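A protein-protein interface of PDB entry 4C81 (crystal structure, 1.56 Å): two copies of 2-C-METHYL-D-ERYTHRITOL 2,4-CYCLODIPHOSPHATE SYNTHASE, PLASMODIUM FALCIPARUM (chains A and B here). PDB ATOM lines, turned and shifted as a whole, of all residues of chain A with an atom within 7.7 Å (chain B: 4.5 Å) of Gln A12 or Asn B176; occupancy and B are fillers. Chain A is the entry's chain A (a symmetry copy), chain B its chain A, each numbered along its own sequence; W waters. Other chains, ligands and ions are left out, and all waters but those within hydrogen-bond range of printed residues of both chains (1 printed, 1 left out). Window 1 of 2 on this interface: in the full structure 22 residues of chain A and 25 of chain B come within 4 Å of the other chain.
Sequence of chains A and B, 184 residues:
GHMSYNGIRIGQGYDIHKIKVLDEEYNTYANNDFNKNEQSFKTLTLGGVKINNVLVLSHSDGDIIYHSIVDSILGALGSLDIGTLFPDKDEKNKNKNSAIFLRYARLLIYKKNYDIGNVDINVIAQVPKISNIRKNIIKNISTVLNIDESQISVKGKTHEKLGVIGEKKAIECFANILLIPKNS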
ATOM      1  N   ILE A  10      18.203  32.122  12.676  1.00  0.00           N
ATOM      2  CA  ILE A  10      18.611  30.719  12.714  1.00  0.00           C
ATOM      3  C   ILE A  10      19.612  30.507  13.845  1.00  0.00           C
ATOM      4  O   ILE A  10      20.482  31.348  14.097  1.00  0.00           O
ATOM      5  CB  ILE A  10      19.250  30.274  11.362  1.00  0.00           C
ATOM      6  CG1 ILE A  10      19.535  28.766  11.346  1.00  0.00           C
ATOM      7  CG2 ILE A  10      20.533  31.042  11.086  1.00  0.00           C
ATOM      8  CD1 ILE A  10      19.923  28.244   9.981  1.00  0.00           C
ATOM      9  N   GLY A  11      19.485  29.368  14.520  1.00  0.00           N
ATOM     10  CA  GLY A  11      20.439  28.960  15.532  1.00  0.00           C
ATOM     11  C   GLY A  11      20.788  27.492  15.414  1.00  0.00           C
ATOM     12  O   GLY A  11      19.947  26.673  15.048  1.00  0.00           O
ATOM     13  N   GLN A  12      22.044  27.170  15.708  1.00  0.00           N
ATOM     14  CA  GLN A  12      22.494  25.789  15.811  1.00  0.00           C
ATOM     15  C   GLN A  12      23.278  25.614  17.099  1.00  0.00           C
ATOM     16  O   GLN A  12      24.226  26.345  17.355  1.00  0.00           O
ATOM     17  CB  GLN A  12      23.379  25.405  14.635  1.00  0.00           C
ATOM     18  CG  GLN A  12      23.788  23.942  14.655  1.00  0.00           C
ATOM     19  CD  GLN A  12      24.708  23.586  13.530  1.00  0.00           C
ATOM     20  OE1 GLN A  12      25.874  23.980  13.522  1.00  0.00           O
ATOM     21  NE2 GLN A  12      24.194  22.832  12.562  1.00  0.00           N
ATOM     22  N   GLY A  13      22.872  24.637  17.898  1.00  0.00           N
ATOM     23  CA  GLY A  13      23.567  24.290  19.120  1.00  0.00           C
ATOM     24  C   GLY A  13      24.234  22.944  18.947  1.00  0.00           C
ATOM     25  O   GLY A  13      23.725  22.080  18.238  1.00  0.00           O
ATOM     26  N   TYR A  14      25.407  22.804  19.551  1.00  0.00           N
ATOM     27  CA  TYR A  14      26.132  21.546  19.555  1.00  0.00           C
ATOM     28  C   TYR A  14      26.529  21.211  20.985  1.00  0.00           C
ATOM     29  O   TYR A  14      26.857  22.099  21.774  1.00  0.00           O
ATOM     30  CB  TYR A  14      27.376  21.653  18.680  1.00  0.00           C
ATOM     31  CG  TYR A  14      28.348  20.515  18.881  1.00  0.00           C
ATOM     32  CD1 TYR A  14      28.143  19.292  18.269  1.00  0.00           C
ATOM     33  CD2 TYR A  14      29.470  20.674  19.690  1.00  0.00           C
ATOM     34  CE1 TYR A  14      29.032  18.241  18.451  1.00  0.00           C
ATOM     35  CE2 TYR A  14      30.369  19.636  19.874  1.00  0.00           C
ATOM     36  CZ  TYR A  14      30.142  18.423  19.253  1.00  0.00           C
ATOM     37  OH  TYR A  14      31.027  17.393  19.443  1.00  0.00           O
ATOM     38  N   SER A  68      22.273  21.666  24.076  1.00  0.00           N
ATOM     39  CA  SER A  68      22.347  22.095  22.677  1.00  0.00           C
ATOM     40  C   SER A  68      21.156  22.978  22.291  1.00  0.00           C
ATOM     41  O   SER A  68      21.317  23.926  21.527  1.00  0.00           O
ATOM     42  CB  SER A  68      22.453  20.897  21.730  1.00  0.00           C
ATOM     43  OG  SER A  68      21.257  20.153  21.701  1.00  0.00           O
ATOM     44  N   ILE A  69      19.973  22.677  22.823  1.00  0.00           N
ATOM     45  CA  ILE A  69      18.800  23.533  22.602  1.00  0.00           C
ATOM     46  C   ILE A  69      19.048  24.948  23.140  1.00  0.00           C
ATOM     47  O   ILE A  69      18.792  25.932  22.443  1.00  0.00           O
ATOM     48  CB  ILE A  69      17.521  22.934  23.235  1.00  0.00           C
ATOM     49  CG1 ILE A  69      17.043  21.724  22.430  1.00  0.00           C
ATOM     50  CG2 ILE A  69      16.402  23.978  23.285  1.00  0.00           C
ATOM     51  CD1 ILE A  69      16.024  20.870  23.155  1.00  0.00           C
ATOM     52  N   VAL A  70      19.561  25.049  24.366  1.00  0.00           N
ATOM     53  CA  VAL A  70      19.876  26.354  24.962  1.00  0.00           C
ATOM     54  C   VAL A  70      20.855  27.133  24.086  1.00  0.00           C
ATOM     55  O   VAL A  70      20.598  28.285  23.743  1.00  0.00           O
ATOM     56  CB  VAL A  70      20.441  26.219  26.389  1.00  0.00           C
ATOM     57  CG1 VAL A  70      20.969  27.558  26.890  1.00  0.00           C
ATOM     58  CG2 VAL A  70      19.368  25.703  27.318  1.00  0.00           C
ATOM     59  N   ASP A  71      21.952  26.499  23.686  1.00  0.00           N
ATOM     60  CA  ASP A  71      22.951  27.193  22.871  1.00  0.00           C
ATOM     61  C   ASP A  71      22.455  27.515  21.459  1.00  0.00           C
ATOM     62  O   ASP A  71      22.944  28.458  20.838  1.00  0.00           O
ATOM     63  CB  ASP A  71      24.277  26.426  22.849  1.00  0.00           C
ATOM     64  CG  ASP A  71      25.093  26.643  24.120  1.00  0.00           C
ATOM     65  OD1 ASP A  71      24.857  27.640  24.842  1.00  0.00           O
ATOM     66  OD2 ASP A  71      25.985  25.818  24.390  1.00  0.00           O
ATOM     67  N   SER A  72      21.476  26.760  20.959  1.00  0.00           N
ATOM     68  CA  SER A  72      20.859  27.088  19.670  1.00  0.00           C
ATOM     69  C   SER A  72      20.065  28.392  19.783  1.00  0.00           C
ATOM     70  O   SER A  72      20.130  29.245  18.899  1.00  0.00           O
ATOM     71  CB  SER A  72      19.979  25.947  19.140  1.00  0.00           C
ATOM     72  OG  SER A  72      18.684  25.930  19.724  1.00  0.00           O
ATOM     73  N   ILE A  73      19.333  28.537  20.880  1.00  0.00           N
ATOM     74  CA  ILE A  73      18.574  29.760  21.162  1.00  0.00           C
ATOM     75  C   ILE A  73      19.499  30.965  21.375  1.00  0.00           C
ATOM     76  O   ILE A  73      19.289  32.024  20.775  1.00  0.00           O
ATOM     77  CB  ILE A  73      17.659  29.567  22.398  1.00  0.00           C
ATOM     78  CG1 ILE A  73      16.546  28.566  22.076  1.00  0.00           C
ATOM     79  CG2 ILE A  73      17.052  30.900  22.846  1.00  0.00           C
ATOM     80  CD1 ILE A  73      15.793  28.078  23.286  1.00  0.00           C
ATOM     81  N   LEU A  74      20.513  30.809  22.225  1.00  0.00           N
ATOM     82  CA  LEU A  74      21.490  31.870  22.466  1.00  0.00           C
ATOM     83  C   LEU A  74      22.193  32.236  21.164  1.00  0.00           C
ATOM     84  O   LEU A  74      22.355  33.414  20.841  1.00  0.00           O
ATOM     85  CB  LEU A  74      22.520  31.434  23.510  1.00  0.00           C
ATOM     86  CG  LEU A  74      21.976  31.271  24.929  1.00  0.00           C
ATOM     87  CD1 LEU A  74      23.059  30.773  25.873  1.00  0.00           C
ATOM     88  CD2 LEU A  74      21.398  32.586  25.415  1.00  0.00           C
ATOM     89  N   GLY A  75      22.597  31.216  20.412  1.00  0.00           N
ATOM     90  CA  GLY A  75      23.263  31.425  19.134  1.00  0.00           C
ATOM     91  C   GLY A  75      22.406  32.210  18.155  1.00  0.00           C
ATOM     92  O   GLY A  75      22.882  33.139  17.497  1.00  0.00           O
ATOM     93  N   ALA A  76      21.133  31.845  18.068  1.00  0.00           N
ATOM     94  CA  ALA A  76      20.189  32.524  17.186  1.00  0.00           C
ATOM     95  C   ALA A  76      20.065  34.017  17.500  1.00  0.00           C
ATOM     96  O   ALA A  76      19.960  34.833  16.584  1.00  0.00           O
ATOM     97  CB  ALA A  76      18.822  31.862  17.270  1.00  0.00           C
ATOM     98  N   ASP A 120      14.617  21.267  15.395  1.00  0.00           N
ATOM     99  CA  ASP A 120      14.922  19.929  14.885  1.00  0.00           C
ATOM    100  C   ASP A 120      16.234  19.493  15.521  1.00  0.00           C
ATOM    101  O   ASP A 120      17.246  20.180  15.402  1.00  0.00           O
ATOM    102  CB  ASP A 120      15.039  19.918  13.354  1.00  0.00           C
ATOM    103  CG  ASP A 120      15.115  18.502  12.772  1.00  0.00           C
ATOM    104  OD1 ASP A 120      14.827  17.522  13.497  1.00  0.00           O
ATOM    105  OD2 ASP A 120      15.454  18.364  11.579  1.00  0.00           O
ATOM    106  N   ASN A 122      19.097  16.471  16.324  1.00  0.00           N
ATOM    107  CA  ASN A 122      19.773  15.265  15.859  1.00  0.00           C
ATOM    108  C   ASN A 122      20.740  14.763  16.915  1.00  0.00           C
ATOM    109  O   ASN A 122      21.750  15.406  17.193  1.00  0.00           O
ATOM    110  CB  ASN A 122      20.557  15.568  14.587  1.00  0.00           C
ATOM    111  CG  ASN A 122      19.665  15.756  13.390  1.00  0.00           C
ATOM    112  OD1 ASN A 122      18.819  14.915  13.106  1.00  0.00           O
ATOM    113  ND2 ASN A 122      19.854  16.856  12.672  1.00  0.00           N
ATOM    114  N   CYS A 173      24.916  15.964  20.108  1.00  0.00           N
ATOM    115  CA  CYS A 173      23.630  16.507  19.683  1.00  0.00           C
ATOM    116  C   CYS A 173      23.850  17.770  18.865  1.00  0.00           C
ATOM    117  O   CYS A 173      24.681  18.608  19.226  1.00  0.00           O
ATOM    118  CB  CYS A 173      22.756  16.839  20.904  1.00  0.00           C
ATOM    119  SG  CYS A 173      21.051  17.267  20.480  1.00  0.00           S
ATOM    120  N   PHE A 174      23.111  17.885  17.761  1.00  0.00           N
ATOM    121  CA  PHE A 174      22.964  19.127  17.014  1.00  0.00           C
ATOM    122  C   PHE A 174      21.514  19.567  17.105  1.00  0.00           C
ATOM    123  O   PHE A 174      20.620  18.824  16.729  1.00  0.00           O
ATOM    124  CB  PHE A 174      23.332  18.930  15.542  1.00  0.00           C
ATOM    125  CG  PHE A 174      24.791  18.717  15.310  1.00  0.00           C
ATOM    126  CD1 PHE A 174      25.353  17.461  15.477  1.00  0.00           C
ATOM    127  CD2 PHE A 174      25.609  19.772  14.933  1.00  0.00           C
ATOM    128  CE1 PHE A 174      26.714  17.256  15.266  1.00  0.00           C
ATOM    129  CE2 PHE A 174      26.967  19.571  14.718  1.00  0.00           C
ATOM    130  CZ  PHE A 174      27.517  18.315  14.888  1.00  0.00           C
ATOM    131  N   ALA A 175      21.285  20.772  17.614  1.00  0.00           N
ATOM    132  CA  ALA A 175      19.942  21.326  17.713  1.00  0.00           C
ATOM    133  C   ALA A 175      19.845  22.508  16.758  1.00  0.00           C
ATOM    134  O   ALA A 175      20.676  23.400  16.809  1.00  0.00           O
ATOM    135  CB  ALA A 175      19.654  21.770  19.138  1.00  0.00           C
ATOM    136  N   ASN A 176      18.830  22.497  15.898  1.00  0.00           N
ATOM    137  CA  ASN A 176      18.627  23.535  14.899  1.00  0.00           C
ATOM    138  C   ASN A 176      17.284  24.194  15.130  1.00  0.00           C
ATOM    139  O   ASN A 176      16.271  23.509  15.265  1.00  0.00           O
ATOM    140  CB  ASN A 176      18.661  22.937  13.497  1.00  0.00           C
ATOM    141  CG  ASN A 176      19.927  22.167  13.233  1.00  0.00           C
ATOM    142  OD1 ASN A 176      20.895  22.715  12.709  1.00  0.00           O
ATOM    143  ND2 ASN A 176      19.943  20.894  13.621  1.00  0.00           N
ATOM    144  N   ILE A 177      17.277  25.521  15.164  1.00  0.00           N
ATOM    145  CA  ILE A 177      16.077  26.263  15.540  1.00  0.00           C
ATOM    146  C   ILE A 177      15.875  27.503  14.676  1.00  0.00           C
ATOM    147  O   ILE A 177      16.836  28.076  14.157  1.00  0.00           O
ATOM    148  CB  ILE A 177      16.157  26.655  17.033  1.00  0.00           C
ATOM    149  CG1 ILE A 177      14.771  26.994  17.583  1.00  0.00           C
ATOM    150  CG2 ILE A 177      17.162  27.785  17.261  1.00  0.00           C
ATOM    151  CD1 ILE A 177      14.741  27.065  19.083  1.00  0.00           C
ATOM    152  N   LEU A 178      14.610  27.887  14.504  1.00  0.00           N
ATOM    153  CA  LEU A 178      14.259  29.177  13.924  1.00  0.00           C
ATOM    154  C   LEU A 178      13.515  29.972  14.980  1.00  0.00           C
ATOM    155  O   LEU A 178      12.636  29.437  15.661  1.00  0.00           O
ATOM    156  CB  LEU A 178      13.352  29.007  12.708  1.00  0.00           C
ATOM    157  CG  LEU A 178      13.998  28.460  11.441  1.00  0.00           C
ATOM    158  CD1 LEU A 178      12.917  28.220  10.398  1.00  0.00           C
ATOM    159  CD2 LEU A 178      15.083  29.386  10.895  1.00  0.00           C
ATOM    160  N   GLY B  11      21.792  28.354   4.648  1.00  0.00           N
ATOM    161  CA  GLY B  11      23.097  27.839   4.284  1.00  0.00           C
ATOM    162  C   GLY B  11      23.835  27.286   5.486  1.00  0.00           C
ATOM    163  O   GLY B  11      23.703  27.798   6.596  1.00  0.00           O
ATOM    164  N   GLN B  12      24.597  26.221   5.257  1.00  0.00           N
ATOM    165  CA  GLN B  12      25.500  25.676   6.260  1.00  0.00           C
ATOM    166  C   GLN B  12      26.866  25.454   5.635  1.00  0.00           C
ATOM    167  O   GLN B  12      26.983  24.789   4.614  1.00  0.00           O
ATOM    168  CB  GLN B  12      24.986  24.354   6.810  1.00  0.00           C
ATOM    169  CG  GLN B  12      25.851  23.802   7.930  1.00  0.00           C
ATOM    170  CD  GLN B  12      25.374  22.472   8.424  1.00  0.00           C
ATOM    171  OE1 GLN B  12      25.507  21.461   7.735  1.00  0.00           O
ATOM    172  NE2 GLN B  12      24.813  22.456   9.629  1.00  0.00           N
ATOM    173  N   ASN B 118      20.870  36.529   9.909  1.00  0.00           N
ATOM    174  CA  ASN B 118      21.901  36.334  10.922  1.00  0.00           C
ATOM    175  C   ASN B 118      22.771  35.133  10.583  1.00  0.00           C
ATOM    176  O   ASN B 118      22.425  34.332   9.716  1.00  0.00           O
ATOM    177  CB  ASN B 118      21.285  36.164  12.310  1.00  0.00           C
ATOM    178  CG  ASN B 118      20.649  34.807  12.500  1.00  0.00           C
ATOM    179  OD1 ASN B 118      19.783  34.406  11.726  1.00  0.00           O
ATOM    180  ND2 ASN B 118      21.089  34.083  13.520  1.00  0.00           N
ATOM    181  N   VAL B 119      23.919  35.050  11.252  1.00  0.00           N
ATOM    182  CA  VAL B 119      24.822  33.911  11.132  1.00  0.00           C
ATOM    183  C   VAL B 119      25.137  33.402  12.545  1.00  0.00           C
ATOM    184  O   VAL B 119      25.319  34.197  13.474  1.00  0.00           O
ATOM    185  CB  VAL B 119      26.116  34.277  10.363  1.00  0.00           C
ATOM    186  CG1 VAL B 119      26.948  35.297  11.128  1.00  0.00           C
ATOM    187  CG2 VAL B 119      26.933  33.026  10.063  1.00  0.00           C
ATOM    188  N   ASP B 120      25.152  32.080  12.704  1.00  0.00           N
ATOM    189  CA  ASP B 120      25.491  31.428  13.970  1.00  0.00           C
ATOM    190  C   ASP B 120      26.606  30.434  13.679  1.00  0.00           C
ATOM    191  O   ASP B 120      26.458  29.556  12.833  1.00  0.00           O
ATOM    192  CB  ASP B 120      24.280  30.710  14.581  1.00  0.00           C
ATOM    193  CG  ASP B 120      24.533  30.227  16.013  1.00  0.00           C
ATOM    194  OD1 ASP B 120      25.533  30.652  16.639  1.00  0.00           O
ATOM    195  OD2 ASP B 120      23.725  29.426  16.525  1.00  0.00           O
ATOM    196  N   ASN B 122      29.596  27.765  15.062  1.00  0.00           N
ATOM    197  CA  ASN B 122      30.013  26.811  16.084  1.00  0.00           C
ATOM    198  C   ASN B 122      31.406  26.290  15.780  1.00  0.00           C
ATOM    199  O   ASN B 122      31.602  25.566  14.806  1.00  0.00           O
ATOM    200  CB  ASN B 122      29.049  25.631  16.116  1.00  0.00           C
ATOM    201  CG  ASN B 122      27.720  25.989  16.725  1.00  0.00           C
ATOM    202  OD1 ASN B 122      27.664  26.535  17.821  1.00  0.00           O
ATOM    203  ND2 ASN B 122      26.638  25.672  16.023  1.00  0.00           N
ATOM    204  N   LYS B 155      30.499  30.794  18.845  1.00  0.00           N
ATOM    205  CA  LYS B 155      30.576  30.004  20.072  1.00  0.00           C
ATOM    206  C   LYS B 155      31.592  28.888  19.869  1.00  0.00           C
ATOM    207  O   LYS B 155      31.735  28.372  18.755  1.00  0.00           O
ATOM    208  CB  LYS B 155      29.209  29.384  20.404  1.00  0.00           C
ATOM    209  CG  LYS B 155      28.000  30.256  20.063  1.00  0.00           C
ATOM    210  CD  LYS B 155      26.693  29.695  20.631  1.00  0.00           C
ATOM    211  CE  LYS B 155      26.229  28.434  19.918  1.00  0.00           C
ATOM    212  NZ  LYS B 155      25.847  28.655  18.495  1.00  0.00           N
ATOM    213  N   PHE B 174      31.220  24.875  12.032  1.00  0.00           N
ATOM    214  CA  PHE B 174      29.947  24.870  11.322  1.00  0.00           C
ATOM    215  C   PHE B 174      29.384  26.280  11.349  1.00  0.00           C
ATOM    216  O   PHE B 174      29.191  26.847  12.415  1.00  0.00           O
ATOM    217  CB  PHE B 174      28.949  23.925  11.993  1.00  0.00           C
ATOM    218  CG  PHE B 174      29.285  22.480  11.828  1.00  0.00           C
ATOM    219  CD1 PHE B 174      30.211  21.875  12.664  1.00  0.00           C
ATOM    220  CD2 PHE B 174      28.686  21.722  10.833  1.00  0.00           C
ATOM    221  CE1 PHE B 174      30.533  20.528  12.514  1.00  0.00           C
ATOM    222  CE2 PHE B 174      29.001  20.377  10.682  1.00  0.00           C
ATOM    223  CZ  PHE B 174      29.926  19.784  11.519  1.00  0.00           C
ATOM    224  N   ALA B 175      29.132  26.846  10.175  1.00  0.00           N
ATOM    225  CA  ALA B 175      28.549  28.176  10.068  1.00  0.00           C
ATOM    226  C   ALA B 175      27.151  28.037   9.482  1.00  0.00           C
ATOM    227  O   ALA B 175      26.986  27.416   8.444  1.00  0.00           O
ATOM    228  CB  ALA B 175      29.409  29.063   9.181  1.00  0.00           C
ATOM    229  N   ASN B 176      26.161  28.613  10.159  1.00  0.00           N
ATOM    230  CA  ASN B 176      24.768  28.533   9.747  1.00  0.00           C
ATOM    231  C   ASN B 176      24.242  29.930   9.495  1.00  0.00           C
ATOM    232  O   ASN B 176      24.401  30.816  10.334  1.00  0.00           O
ATOM    233  CB  ASN B 176      23.932  27.867  10.833  1.00  0.00           C
ATOM    234  CG  ASN B 176      24.465  26.513  11.218  1.00  0.00           C
ATOM    235  OD1 ASN B 176      24.042  25.496  10.672  1.00  0.00           O
ATOM    236  ND2 ASN B 176      25.423  26.490  12.141  1.00  0.00           N
ATOM    237  N   ILE B 177      23.604  30.120   8.347  1.00  0.00           N
ATOM    238  CA  ILE B 177      23.195  31.455   7.919  1.00  0.00           C
ATOM    239  C   ILE B 177      21.812  31.454   7.278  1.00  0.00           C
ATOM    240  O   ILE B 177      21.378  30.448   6.711  1.00  0.00           O
ATOM    241  CB  ILE B 177      24.242  32.028   6.937  1.00  0.00           C
ATOM    242  CG1 ILE B 177      24.123  33.549   6.839  1.00  0.00           C
ATOM    243  CG2 ILE B 177      24.153  31.351   5.568  1.00  0.00           C
ATOM    244  CD1 ILE B 177      25.305  34.184   6.162  1.00  0.00           C
HETATM  245  O   HOH W   1      26.727  25.158  20.353  1.00  0.00           O
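Water W1 bridges N of Tyr A14 and OD1 of Asn B122.
NE2 of Gln A12 sits close to NE2 of Gln B12, at 3.0 Å.
The side-chain amide nitrogen of Asn B118 sits at hydrogen-bond distance from the backbone carbonyl oxygen of Ile A10, 2.9 Å away.
ND2 of Asn B118 sits at hydrogen-bond distance from O of Ala A76, at 3.4 Å.
The side-chain carboxylate (OD2) of Asp B120 sits at hydrogen-bond distance from the backbone NH (N) of Gln A12 (2.9 Å).
The side-chain amide nitrogen (ND2) of Asn B122 is in hydrogen-bond range of the backbone carbonyl oxygen (O) of Gln A12, at 2.8 Å.
The backbone carbonyl oxygen (O) of Gln A12 sits at hydrogen-bond distance from the side-chain amino group (NZ) of Lys B155.
ND2 of Asn B176 sits at hydrogen-bond distance from OE1 of Gln A12, 2.9 Å away.
Of the 11 printed residues of chain B, 7 touch a printed residue of chain A.
Printed residues of chain A that touch a printed residue of chain B: Ile A10, Gly A11, Gln A12, Asp A71, Gly A75 and Ala A76.
Hydrophobic or aromatic side chains of chain A within 4 Å of the printed part of chain B: Ile A10.
Along chain A the printed residues that touch a printed residue of chain B span positions 10 to 76.
Gly A11 touches Asp B120, but with the chains exchanged Asp A120 does not touch Gly B11 (13.3 Å).
Gln A12 touches its own counterpart, Gln B12.
Gln A12 touches Asp B120, but with the chains exchanged Asp A120 does not touch Gln B12 (9.8 Å).
Gln A12 touches Phe B174, but with the chains exchanged Phe A174 does not touch Gln B12 (6.0 Å).
Positions printed for both chains: 11, 12, 120, 122, 174, 175, 176 and 177.
The side-chain amide oxygen (OD1) of Asn B176 is in hydrogen-bond range of the side-chain amide nitrogen (NE2) of Gln B12, at 3.3 Å.
The side-chain carboxylate (OD1) of Asp B120 lies within salt-bridge range of the side-chain amino group (NZ) of Lys B155, 2.7 Å away.
The backbone carbonyl oxygen (O) of Asn B176 sits at hydrogen-bond distance from the backbone NH (N) of Asp B120, 2.8 Å away.
The side-chain amino group (NZ) of Lys B155 lies within hydrogen-bond range of the side-chain amide oxygen (OD1) of Asn B122 (2.9 Å).
The backbone carbonyl oxygen of Gly A11 lies within hydrogen-bond range of the backbone NH of Ile A177 (2.9 Å).
The side-chain amide oxygen (OD1) of Asn A176 is in hydrogen-bond range of the side-chain amide nitrogen (NE2) of Gln A12 (3.3 Å).
Gln A12 touches just these residues of chain B: Gln B12 (3.0 Å), Asp B120 (2.9 Å), Asn B122 (2.8 Å), Lys B155 (3.0 Å), Phe B174 (3.4 Å) and Asn B176 (2.9 Å).
Asn B176 touches two residues of chain A.
No residue of chain A comes within 4 Å of Ala B175.
Of the printed residues of chain A, Lys B155 touches Gln A12 (3.0 Å), Asp A71 (3.4 Å) and Gly A75 (3.8 Å).
Of the printed residues of chain A, Phe B174 touches Gln A12.
Printed residues of chain B within 4 Å of Gly A11: Asp B120 (3.5 Å).
Of the printed residues of chain A, Asn B118 touches Ile A10 (2.9 Å) and Ala A76 (3.4 Å).
The nearest printed residue of chain A that does not touch Asp B120 is Ser A72 (4.3 Å).
Ile A10 touches Asp B120 (O to CB, 3.9 Å).
Asn B176 touches Ile A10.
Gly A11 touches Asp B120 (CA to OD2, 3.5 Å).
Gln A12 touches Phe B174.
O of Asp A71 touches CE of Lys B155, 3.4 Å away.
Gly A75 touches Asp B120 (CA to OD2, 3.3 Å).
NZ of Lys B155 touches CA of Gly A75 (3.8 Å).
Asp B120 touches Ala A76 (OD2 to N, 3.9 Å).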
